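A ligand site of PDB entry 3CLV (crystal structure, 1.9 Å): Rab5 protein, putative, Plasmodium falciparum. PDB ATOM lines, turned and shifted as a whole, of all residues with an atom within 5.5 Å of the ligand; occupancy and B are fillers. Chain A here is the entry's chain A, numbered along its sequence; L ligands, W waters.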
ATOM      1  N   GLY A  14     -22.915  29.634 -24.581  1.00  0.00           N
ATOM      2  CA  GLY A  14     -22.376  28.488 -23.828  1.00  0.00           C
ATOM      3  C   GLY A  14     -22.383  28.826 -22.356  1.00  0.00           C
ATOM      4  O   GLY A  14     -22.502  30.002 -21.986  1.00  0.00           O
ATOM      5  N   GLU A  15     -22.261  27.808 -21.509  1.00  0.00           N
ATOM      6  CA  GLU A  15     -22.248  28.005 -20.049  1.00  0.00           C
ATOM      7  C   GLU A  15     -21.022  28.857 -19.640  1.00  0.00           C
ATOM      8  O   GLU A  15     -19.991  28.802 -20.319  1.00  0.00           O
ATOM      9  CB  GLU A  15     -22.213  26.633 -19.357  1.00  0.00           C
ATOM     10  CG  GLU A  15     -22.213  26.687 -17.821  1.00  0.00           C
ATOM     11  CD  GLU A  15     -22.397  25.327 -17.155  1.00  0.00           C
ATOM     12  OE1 GLU A  15     -22.987  24.401 -17.781  1.00  0.00           O
ATOM     13  OE2 GLU A  15     -21.944  25.202 -15.992  1.00  0.00           O
ATOM     14  N   SER A  16     -21.111  29.645 -18.575  1.00  0.00           N
ATOM     15  CA  SER A  16     -19.905  30.317 -18.081  1.00  0.00           C
ATOM     16  C   SER A  16     -18.768  29.334 -17.832  1.00  0.00           C
ATOM     17  O   SER A  16     -18.979  28.184 -17.393  1.00  0.00           O
ATOM     18  CB  SER A  16     -20.152  31.208 -16.854  1.00  0.00           C
ATOM     19  OG  SER A  16     -20.640  30.443 -15.764  1.00  0.00           O
ATOM     20  N   SER A  17     -17.557  29.804 -18.165  1.00  0.00           N
ATOM     21  CA  SER A  17     -16.284  29.098 -17.999  1.00  0.00           C
ATOM     22  C   SER A  17     -15.863  28.206 -19.164  1.00  0.00           C
ATOM     23  O   SER A  17     -14.744  27.695 -19.145  1.00  0.00           O
ATOM     24  CB  SER A  17     -16.212  28.303 -16.679  1.00  0.00           C
ATOM     25  OG  SER A  17     -16.718  26.989 -16.877  1.00  0.00           O
ATOM     26  N   VAL A  18     -16.741  28.026 -20.164  1.00  0.00           N
ATOM     27  CA  VAL A  18     -16.407  27.172 -21.333  1.00  0.00           C
ATOM     28  C   VAL A  18     -15.364  27.767 -22.257  1.00  0.00           C
ATOM     29  O   VAL A  18     -14.691  27.054 -22.998  1.00  0.00           O
ATOM     30  CB  VAL A  18     -17.663  26.696 -22.137  1.00  0.00           C
ATOM     31  CG1 VAL A  18     -18.621  25.956 -21.221  1.00  0.00           C
ATOM     32  CG2 VAL A  18     -18.359  27.849 -22.882  1.00  0.00           C
ATOM     33  N   GLY A  19     -15.195  29.091 -22.214  1.00  0.00           N
ATOM     34  CA  GLY A  19     -14.124  29.726 -22.964  1.00  0.00           C
ATOM     35  C   GLY A  19     -14.545  30.686 -24.065  1.00  0.00           C
ATOM     36  O   GLY A  19     -13.741  30.994 -24.952  1.00  0.00           O
ATOM     37  N   LYS A  20     -15.776  31.184 -24.011  1.00  0.00           N
ATOM     38  CA  LYS A  20     -16.269  32.160 -25.006  1.00  0.00           C
ATOM     39  C   LYS A  20     -15.401  33.424 -25.084  1.00  0.00           C
ATOM     40  O   LYS A  20     -15.012  33.831 -26.170  1.00  0.00           O
ATOM     41  CB  LYS A  20     -17.727  32.544 -24.691  1.00  0.00           C
ATOM     42  CG  LYS A  20     -18.732  31.376 -24.751  1.00  0.00           C
ATOM     43  CD  LYS A  20     -20.184  31.853 -24.473  1.00  0.00           C
ATOM     44  CE  LYS A  20     -20.426  32.464 -23.062  1.00  0.00           C
ATOM     45  NZ  LYS A  20     -20.028  31.572 -21.871  1.00  0.00           N
ATOM     46  N   SER A  21     -15.070  34.038 -23.943  1.00  0.00           N
ATOM     47  CA  SER A  21     -14.300  35.297 -24.028  1.00  0.00           C
ATOM     48  C   SER A  21     -12.913  34.986 -24.577  1.00  0.00           C
ATOM     49  O   SER A  21     -12.341  35.790 -25.289  1.00  0.00           O
ATOM     50  CB  SER A  21     -14.217  36.037 -22.670  1.00  0.00           C
ATOM     51  OG  SER A  21     -13.292  35.436 -21.776  1.00  0.00           O
ATOM     52  N   SER A  22     -12.411  33.791 -24.259  1.00  0.00           N
ATOM     53  CA  SER A  22     -11.101  33.326 -24.727  1.00  0.00           C
ATOM     54  C   SER A  22     -11.080  33.060 -26.226  1.00  0.00           C
ATOM     55  O   SER A  22     -10.115  33.406 -26.910  1.00  0.00           O
ATOM     56  CB  SER A  22     -10.654  32.111 -23.931  1.00  0.00           C
ATOM     57  OG  SER A  22     -10.556  32.427 -22.543  1.00  0.00           O
ATOM     58  N   ILE A  23     -12.151  32.445 -26.759  1.00  0.00           N
ATOM     59  CA  ILE A  23     -12.274  32.306 -28.205  1.00  0.00           C
ATOM     60  C   ILE A  23     -12.210  33.668 -28.890  1.00  0.00           C
ATOM     61  O   ILE A  23     -11.498  33.840 -29.888  1.00  0.00           O
ATOM     62  CB  ILE A  23     -13.568  31.529 -28.597  1.00  0.00           C
ATOM     63  CG1 ILE A  23     -13.478  30.087 -28.134  1.00  0.00           C
ATOM     64  CG2 ILE A  23     -13.850  31.598 -30.130  1.00  0.00           C
ATOM     65  CD1 ILE A  23     -14.836  29.335 -28.149  1.00  0.00           C
ATOM     66  N   PHE A  32      -4.086  34.829 -25.250  1.00  0.00           N
ATOM     67  CA  PHE A  32      -4.805  34.013 -24.278  1.00  0.00           C
ATOM     68  C   PHE A  32      -4.472  34.423 -22.840  1.00  0.00           C
ATOM     69  O   PHE A  32      -3.299  34.622 -22.500  1.00  0.00           O
ATOM     70  CB  PHE A  32      -4.512  32.516 -24.513  1.00  0.00           C
ATOM     71  CG  PHE A  32      -5.096  31.598 -23.473  1.00  0.00           C
ATOM     72  CD1 PHE A  32      -6.438  31.202 -23.529  1.00  0.00           C
ATOM     73  CD2 PHE A  32      -4.306  31.109 -22.445  1.00  0.00           C
ATOM     74  CE1 PHE A  32      -6.970  30.352 -22.555  1.00  0.00           C
ATOM     75  CE2 PHE A  32      -4.822  30.231 -21.490  1.00  0.00           C
ATOM     76  CZ  PHE A  32      -6.158  29.856 -21.545  1.00  0.00           C
ATOM     77  N   HIS A  33      -5.517  34.516 -22.000  1.00  0.00           N
ATOM     78  CA  HIS A  33      -5.363  34.762 -20.559  1.00  0.00           C
ATOM     79  C   HIS A  33      -5.819  33.558 -19.748  1.00  0.00           C
ATOM     80  O   HIS A  33      -6.970  33.142 -19.871  1.00  0.00           O
ATOM     81  CB  HIS A  33      -6.150  36.014 -20.115  1.00  0.00           C
ATOM     82  CG  HIS A  33      -5.754  37.278 -20.819  1.00  0.00           C
ATOM     83  ND1 HIS A  33      -6.600  38.362 -20.924  1.00  0.00           N
ATOM     84  CD2 HIS A  33      -4.607  37.631 -21.460  1.00  0.00           C
ATOM     85  CE1 HIS A  33      -5.989  39.329 -21.579  1.00  0.00           C
ATOM     86  NE2 HIS A  33      -4.784  38.907 -21.914  1.00  0.00           N
ATOM     87  N   GLU A  34      -4.907  33.027 -18.903  1.00  0.00           N
ATOM     88  CA  GLU A  34      -5.196  31.858 -18.069  1.00  0.00           C
ATOM     89  C   GLU A  34      -6.259  32.165 -17.005  1.00  0.00           C
ATOM     90  O   GLU A  34      -6.951  31.262 -16.524  1.00  0.00           O
ATOM     91  CB  GLU A  34      -3.923  31.312 -17.409  1.00  0.00           C
ATOM     92  CG  GLU A  34      -2.871  30.761 -18.379  1.00  0.00           C
ATOM     93  CD  GLU A  34      -3.040  29.274 -18.717  1.00  0.00           C
ATOM     94  OE1 GLU A  34      -2.120  28.718 -19.346  1.00  0.00           O
ATOM     95  OE2 GLU A  34      -4.069  28.663 -18.364  1.00  0.00           O
ATOM     96  N   ASN A  35      -6.367  33.442 -16.641  1.00  0.00           N
ATOM     97  CA  ASN A  35      -7.372  33.924 -15.689  1.00  0.00           C
ATOM     98  C   ASN A  35      -8.228  34.963 -16.408  1.00  0.00           C
ATOM     99  O   ASN A  35      -7.711  35.766 -17.154  1.00  0.00           O
ATOM    100  CB  ASN A  35      -6.692  34.594 -14.491  1.00  0.00           C
ATOM    101  CG  ASN A  35      -5.742  33.657 -13.753  1.00  0.00           C
ATOM    102  OD1 ASN A  35      -6.008  32.474 -13.610  1.00  0.00           O
ATOM    103  ND2 ASN A  35      -4.611  34.199 -13.318  1.00  0.00           N
ATOM    104  N   THR A  36      -9.541  34.909 -16.183  1.00  0.00           N
ATOM    105  CA  THR A  36     -10.454  35.846 -16.848  1.00  0.00           C
ATOM    106  C   THR A  36     -11.438  36.384 -15.823  1.00  0.00           C
ATOM    107  O   THR A  36     -11.650  35.752 -14.800  1.00  0.00           O
ATOM    108  CB  THR A  36     -11.227  35.193 -18.043  1.00  0.00           C
ATOM    109  OG1 THR A  36     -12.047  34.122 -17.565  1.00  0.00           O
ATOM    110  CG2 THR A  36     -10.275  34.676 -19.120  1.00  0.00           C
ATOM    111  N   ASN A  37     -12.020  37.540 -16.098  1.00  0.00           N
ATOM    112  CA  ASN A  37     -12.971  38.167 -15.189  1.00  0.00           C
ATOM    113  C   ASN A  37     -14.372  38.105 -15.793  1.00  0.00           C
ATOM    114  O   ASN A  37     -14.524  37.903 -16.992  1.00  0.00           O
ATOM    115  CB  ASN A  37     -12.606  39.642 -14.907  1.00  0.00           C
ATOM    116  CG  ASN A  37     -11.186  39.826 -14.340  1.00  0.00           C
ATOM    117  OD1 ASN A  37     -10.631  40.928 -14.404  1.00  0.00           O
ATOM    118  ND2 ASN A  37     -10.607  38.771 -13.801  1.00  0.00           N
ATOM    119  N   ASP A  99     -21.324  37.895 -27.761  1.00  0.00           N
ATOM    120  CA  ASP A  99     -20.998  36.918 -26.708  1.00  0.00           C
ATOM    121  C   ASP A  99     -21.989  37.085 -25.572  1.00  0.00           C
ATOM    122  O   ASP A  99     -22.023  38.133 -24.927  1.00  0.00           O
ATOM    123  CB  ASP A  99     -19.559  37.119 -26.218  1.00  0.00           C
ATOM    124  CG  ASP A  99     -19.164  36.192 -25.069  1.00  0.00           C
ATOM    125  OD1 ASP A  99     -19.923  35.253 -24.734  1.00  0.00           O
ATOM    126  OD2 ASP A  99     -18.051  36.412 -24.512  1.00  0.00           O
ATOM    127  N   ASN A 155     -14.504  23.058 -26.880  1.00  0.00           N
ATOM    128  CA  ASN A 155     -13.331  23.822 -26.477  1.00  0.00           C
ATOM    129  C   ASN A 155     -12.520  23.154 -25.341  1.00  0.00           C
ATOM    130  O   ASN A 155     -13.035  22.310 -24.606  1.00  0.00           O
ATOM    131  CB  ASN A 155     -13.730  25.270 -26.110  1.00  0.00           C
ATOM    132  CG  ASN A 155     -12.528  26.211 -26.001  1.00  0.00           C
ATOM    133  OD1 ASN A 155     -11.664  26.260 -26.891  1.00  0.00           O
ATOM    134  ND2 ASN A 155     -12.497  27.012 -24.937  1.00  0.00           N
ATOM    135  N   LYS A 156     -11.246  23.554 -25.240  1.00  0.00           N
ATOM    136  CA  LYS A 156     -10.311  23.105 -24.180  1.00  0.00           C
ATOM    137  C   LYS A 156      -9.703  21.728 -24.430  1.00  0.00           C
ATOM    138  O   LYS A 156      -9.310  21.025 -23.486  1.00  0.00           O
ATOM    139  CB  LYS A 156     -10.941  23.177 -22.780  1.00  0.00           C
ATOM    140  CG  LYS A 156     -11.582  24.551 -22.462  1.00  0.00           C
ATOM    141  CD  LYS A 156     -11.558  24.762 -20.961  1.00  0.00           C
ATOM    142  CE  LYS A 156     -12.543  25.843 -20.525  1.00  0.00           C
ATOM    143  NZ  LYS A 156     -12.415  26.151 -19.055  1.00  0.00           N
ATOM    144  N   ILE A 157      -9.601  21.355 -25.705  1.00  0.00           N
ATOM    145  CA  ILE A 157      -9.059  20.048 -26.068  1.00  0.00           C
ATOM    146  C   ILE A 157      -7.599  19.869 -25.646  1.00  0.00           C
ATOM    147  O   ILE A 157      -7.112  18.734 -25.558  1.00  0.00           O
ATOM    148  CB  ILE A 157      -9.219  19.718 -27.582  1.00  0.00           C
ATOM    149  CG1 ILE A 157      -8.410  20.698 -28.433  1.00  0.00           C
ATOM    150  CG2 ILE A 157     -10.722  19.632 -27.933  1.00  0.00           C
ATOM    151  CD1 ILE A 157      -8.325  20.357 -29.889  1.00  0.00           C
ATOM    152  N   ASP A 158      -6.908  20.990 -25.360  1.00  0.00           N
ATOM    153  CA  ASP A 158      -5.540  20.953 -24.831  1.00  0.00           C
ATOM    154  C   ASP A 158      -5.464  20.284 -23.447  1.00  0.00           C
ATOM    155  O   ASP A 158      -4.391  19.861 -23.029  1.00  0.00           O
ATOM    156  CB  ASP A 158      -4.981  22.363 -24.737  1.00  0.00           C
ATOM    157  CG  ASP A 158      -5.782  23.229 -23.791  1.00  0.00           C
ATOM    158  OD1 ASP A 158      -5.501  23.202 -22.568  1.00  0.00           O
ATOM    159  OD2 ASP A 158      -6.698  23.921 -24.262  1.00  0.00           O
ATOM    160  N   LYS A 159      -6.585  20.228 -22.737  1.00  0.00           N
ATOM    161  CA  LYS A 159      -6.599  19.605 -21.409  1.00  0.00           C
ATOM    162  C   LYS A 159      -6.508  18.075 -21.489  1.00  0.00           C
ATOM    163  O   LYS A 159      -6.833  17.473 -22.529  1.00  0.00           O
ATOM    164  CB  LYS A 159      -7.826  20.060 -20.614  1.00  0.00           C
ATOM    165  CG  LYS A 159      -7.817  21.553 -20.227  1.00  0.00           C
ATOM    166  CD  LYS A 159      -9.086  21.943 -19.487  1.00  0.00           C
ATOM    167  CE  LYS A 159      -9.017  21.505 -18.038  1.00  0.00           C
ATOM    168  NZ  LYS A 159     -10.161  21.977 -17.216  1.00  0.00           N
ATOM    169  N   THR A 183     -11.642  22.661 -30.484  1.00  0.00           N
ATOM    170  CA  THR A 183     -10.774  23.844 -30.404  1.00  0.00           C
ATOM    171  C   THR A 183     -10.003  23.956 -29.082  1.00  0.00           C
ATOM    172  O   THR A 183     -10.356  23.346 -28.069  1.00  0.00           O
ATOM    173  CB  THR A 183     -11.589  25.179 -30.601  1.00  0.00           C
ATOM    174  OG1 THR A 183     -12.511  25.343 -29.531  1.00  0.00           O
ATOM    175  CG2 THR A 183     -12.323  25.210 -31.937  1.00  0.00           C
ATOM    176  N   SER A 184      -8.933  24.746 -29.127  1.00  0.00           N
ATOM    177  CA  SER A 184      -8.282  25.252 -27.925  1.00  0.00           C
ATOM    178  C   SER A 184      -8.012  26.747 -28.100  1.00  0.00           C
ATOM    179  O   SER A 184      -7.263  27.159 -28.979  1.00  0.00           O
ATOM    180  CB  SER A 184      -6.996  24.465 -27.590  1.00  0.00           C
ATOM    181  OG  SER A 184      -6.367  24.992 -26.409  1.00  0.00           O
ATOM    182  N   ALA A 185      -8.667  27.558 -27.266  1.00  0.00           N
ATOM    183  CA  ALA A 185      -8.323  28.987 -27.167  1.00  0.00           C
ATOM    184  C   ALA A 185      -6.907  29.150 -26.630  1.00  0.00           C
ATOM    185  O   ALA A 185      -6.202  30.073 -26.999  1.00  0.00           O
ATOM    186  CB  ALA A 185      -9.314  29.718 -26.258  1.00  0.00           C
ATOM    187  N   LYS A 186      -6.500  28.236 -25.750  1.00  0.00           N
ATOM    188  CA  LYS A 186      -5.154  28.268 -25.151  1.00  0.00           C
ATOM    189  C   LYS A 186      -4.036  28.140 -26.207  1.00  0.00           C
ATOM    190  O   LYS A 186      -3.137  28.980 -26.263  1.00  0.00           O
ATOM    191  CB  LYS A 186      -5.016  27.224 -24.023  1.00  0.00           C
ATOM    192  CG  LYS A 186      -3.712  27.341 -23.194  1.00  0.00           C
ATOM    193  CD  LYS A 186      -3.655  26.343 -22.040  1.00  0.00           C
ATOM    194  CE  LYS A 186      -2.242  26.271 -21.419  1.00  0.00           C
ATOM    195  NZ  LYS A 186      -2.313  25.435 -20.170  1.00  0.00           N
HETATM  196  P1  LIG L   1     -16.524  32.174 -20.742  1.00  0.00           P
HETATM  197  O1  LIG L   1     -16.412  33.468 -21.465  1.00  0.00           O
HETATM  198  O2  LIG L   1     -17.204  32.351 -19.403  1.00  0.00           O
HETATM  199  O3  LIG L   1     -17.275  31.124 -21.523  1.00  0.00           O
HETATM  200  O4  LIG L   1     -15.053  31.525 -20.491  1.00  0.00           O
HETATM  201  P2  LIG L   1     -13.658  32.354 -20.351  1.00  0.00           P
HETATM  202  O5  LIG L   1     -13.787  33.423 -19.282  1.00  0.00           O
HETATM  203  O6  LIG L   1     -13.121  32.836 -21.655  1.00  0.00           O
HETATM  204  O7  LIG L   1     -12.693  31.202 -19.787  1.00  0.00           O
HETATM  205  C1  LIG L   1     -12.922  30.564 -18.515  1.00  0.00           C
HETATM  206  C2  LIG L   1     -11.589  29.953 -18.053  1.00  0.00           C
HETATM  207  O8  LIG L   1     -11.206  28.890 -18.913  1.00  0.00           O
HETATM  208  C3  LIG L   1     -10.411  30.924 -18.025  1.00  0.00           C
HETATM  209  O9  LIG L   1      -9.634  30.531 -16.885  1.00  0.00           O
HETATM  210  C4  LIG L   1      -9.624  30.616 -19.299  1.00  0.00           C
HETATM  211  O10 LIG L   1      -8.209  30.888 -19.201  1.00  0.00           O
HETATM  212  C5  LIG L   1      -9.879  29.121 -19.433  1.00  0.00           C
HETATM  213  N1  LIG L   1      -9.886  28.682 -20.828  1.00  0.00           N
HETATM  214  C6  LIG L   1     -10.623  29.216 -21.831  1.00  0.00           C
HETATM  215  N2  LIG L   1     -10.384  28.557 -22.983  1.00  0.00           N
HETATM  216  C7  LIG L   1      -9.490  27.577 -22.711  1.00  0.00           C
HETATM  217  C8  LIG L   1      -8.808  26.504 -23.470  1.00  0.00           C
HETATM  218  O11 LIG L   1      -9.040  26.363 -24.694  1.00  0.00           O
HETATM  219  N3  LIG L   1      -7.944  25.692 -22.795  1.00  0.00           N
HETATM  220  C9  LIG L   1      -7.691  25.817 -21.470  1.00  0.00           C
HETATM  221  N4  LIG L   1      -6.825  24.958 -20.887  1.00  0.00           N
HETATM  222  N5  LIG L   1      -8.270  26.796 -20.707  1.00  0.00           N
HETATM  223  C10 LIG L   1      -9.166  27.668 -21.272  1.00  0.00           C
HETATM  224  O   HOH W   1     -14.477  30.959 -15.519  1.00  0.00           O
HETATM  225  O   HOH W   2     -15.064  35.862 -19.035  1.00  0.00           O
HETATM  226  O   HOH W   3      -6.415  28.600 -17.783  1.00  0.00           O
HETATM  227  O   HOH W   4      -9.782  25.952 -17.977  1.00  0.00           O
HETATM  228  O   HOH W   5      -7.883  30.447 -13.993  1.00  0.00           O
HETATM  229  O   HOH W   6     -17.823  35.546 -22.169  1.00  0.00           O
HETATM  230  O   HOH W   7      -9.893  27.674 -15.889  1.00  0.00           O
HETATM  231  O   HOH W   8     -18.820  34.293 -18.791  1.00  0.00           O
HETATM  232  O   HOH W   9     -15.944  32.687 -16.927  1.00  0.00           O
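An oxygen (O5) of the ligand is in hydrogen-bond range of the side-chain hydroxyl (OG1) of Thr 36, at 2.5 Å.
N of Ser 21 is in hydrogen-bond range of O1 of the ligand, at 2.9 Å.
The side-chain hydroxyl of Ser 21 is in hydrogen-bond range of an oxygen (O6) of the ligand (2.6 Å).
The side-chain carboxylate of Asp 158 lies within hydrogen-bond range of a nitrogen (N3) of the ligand.
The backbone carbonyl oxygen of His 33 is in hydrogen-bond range of an oxygen (O10) of the ligand (2.7 Å).
O6 of the ligand lies within hydrogen-bond range of N of Ser 22 (2.9 Å).
An oxygen (O6) of the ligand is in hydrogen-bond range of the side-chain hydroxyl (OG) of Ser 22, 2.7 Å away.
An oxygen (O9) of the ligand is in hydrogen-bond range of the backbone carbonyl oxygen of Glu 34 (2.8 Å).
O3 of the ligand is in hydrogen-bond range of N of Lys 20 (2.9 Å).
An oxygen (O3) of the ligand is in salt-bridge range of the side-chain amino group (NZ) of Lys 20, at 2.8 Å.
N of Ser 17 lies within hydrogen-bond range of O2 of the ligand (2.9 Å).
O11 of the ligand is in hydrogen-bond range of N of Ala 185 (2.9 Å).
N of Gly 19 sits at hydrogen-bond distance from O4 of the ligand, 3.0 Å away.
The side-chain amino group (NZ) of Lys 156 sits at hydrogen-bond distance from an oxygen (O8) of the ligand (3.0 Å).
N2 of the ligand sits at hydrogen-bond distance from ND2 of Asn 155 (3.3 Å).
An oxygen (O11) of the ligand lies within hydrogen-bond range of the backbone NH (N) of Lys 186, at 3.3 Å.
N of Val 18 sits at hydrogen-bond distance from O3 of the ligand.
The side-chain hydroxyl (OG) of Ser 184 lies within hydrogen-bond range of an oxygen (O11) of the ligand (3.5 Å).
The side-chain carboxylate of Asp 158 lies within hydrogen-bond range of the side-chain hydroxyl of Ser 184, at 2.4 Å.
OE1 of Glu 34 lies within salt-bridge range of NZ of Lys 186 (3.4 Å).
The side-chain amino group (NZ) of Lys 20 sits at hydrogen-bond distance from the backbone carbonyl oxygen (O) of Gly 14 (2.9 Å).
The backbone carbonyl oxygen (O) of Ser 17 lies within hydrogen-bond range of the side-chain amino group (NZ) of Lys 156 (2.8 Å).
The backbone NH of Ala 185 is in hydrogen-bond range of the side-chain amide oxygen of Asn 155 (3.3 Å).
The backbone NH (N) of Lys 156 lies within hydrogen-bond range of the backbone carbonyl oxygen (O) of Thr 183 (3.0 Å).
O of Val 18 sits at hydrogen-bond distance from ND2 of Asn 155.
OD1 of Asn 155 lies within hydrogen-bond range of OG1 of Thr 183 (2.9 Å).
Glu 15 touches the ligand.
CA of Ser 16 touches O2 of the ligand, 3.6 Å away.
Phe 32 touches the ligand (CZ to O10, 3.3 Å).
CG of Lys 159 touches N4 of the ligand, at 3.6 Å.
Hydrophobic or aromatic side chains within 4 Å of the ligand: Val 18, Phe 32 and Ala 185.
The nearest printed residue that does not touch the ligand is Asn 35 (4.1 Å).
Water W6 lies within hydrogen-bond range of OD2 of Asp 99 and O1 of the ligand.
Water W2 lies within hydrogen-bond range of an oxygen (O5) of the ligand (2.8 Å), the backbone carbonyl oxygen of Asn 37 (2.9 Å) and the side-chain hydroxyl of Ser 21 (3.3 Å).
Water W4 bridges the side-chain amino group (NZ) of Lys 156 (2.9 Å) and a nitrogen (N5) of the ligand (3.2 Å).
Water W3 lies within hydrogen-bond range of the side-chain carboxylate of Glu 34 (2.4 Å) and an oxygen (O10) of the ligand (3.2 Å).
Water W5 lies within hydrogen-bond range of OD1 of Asn 35, O of Glu 34 and O9 of the ligand.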
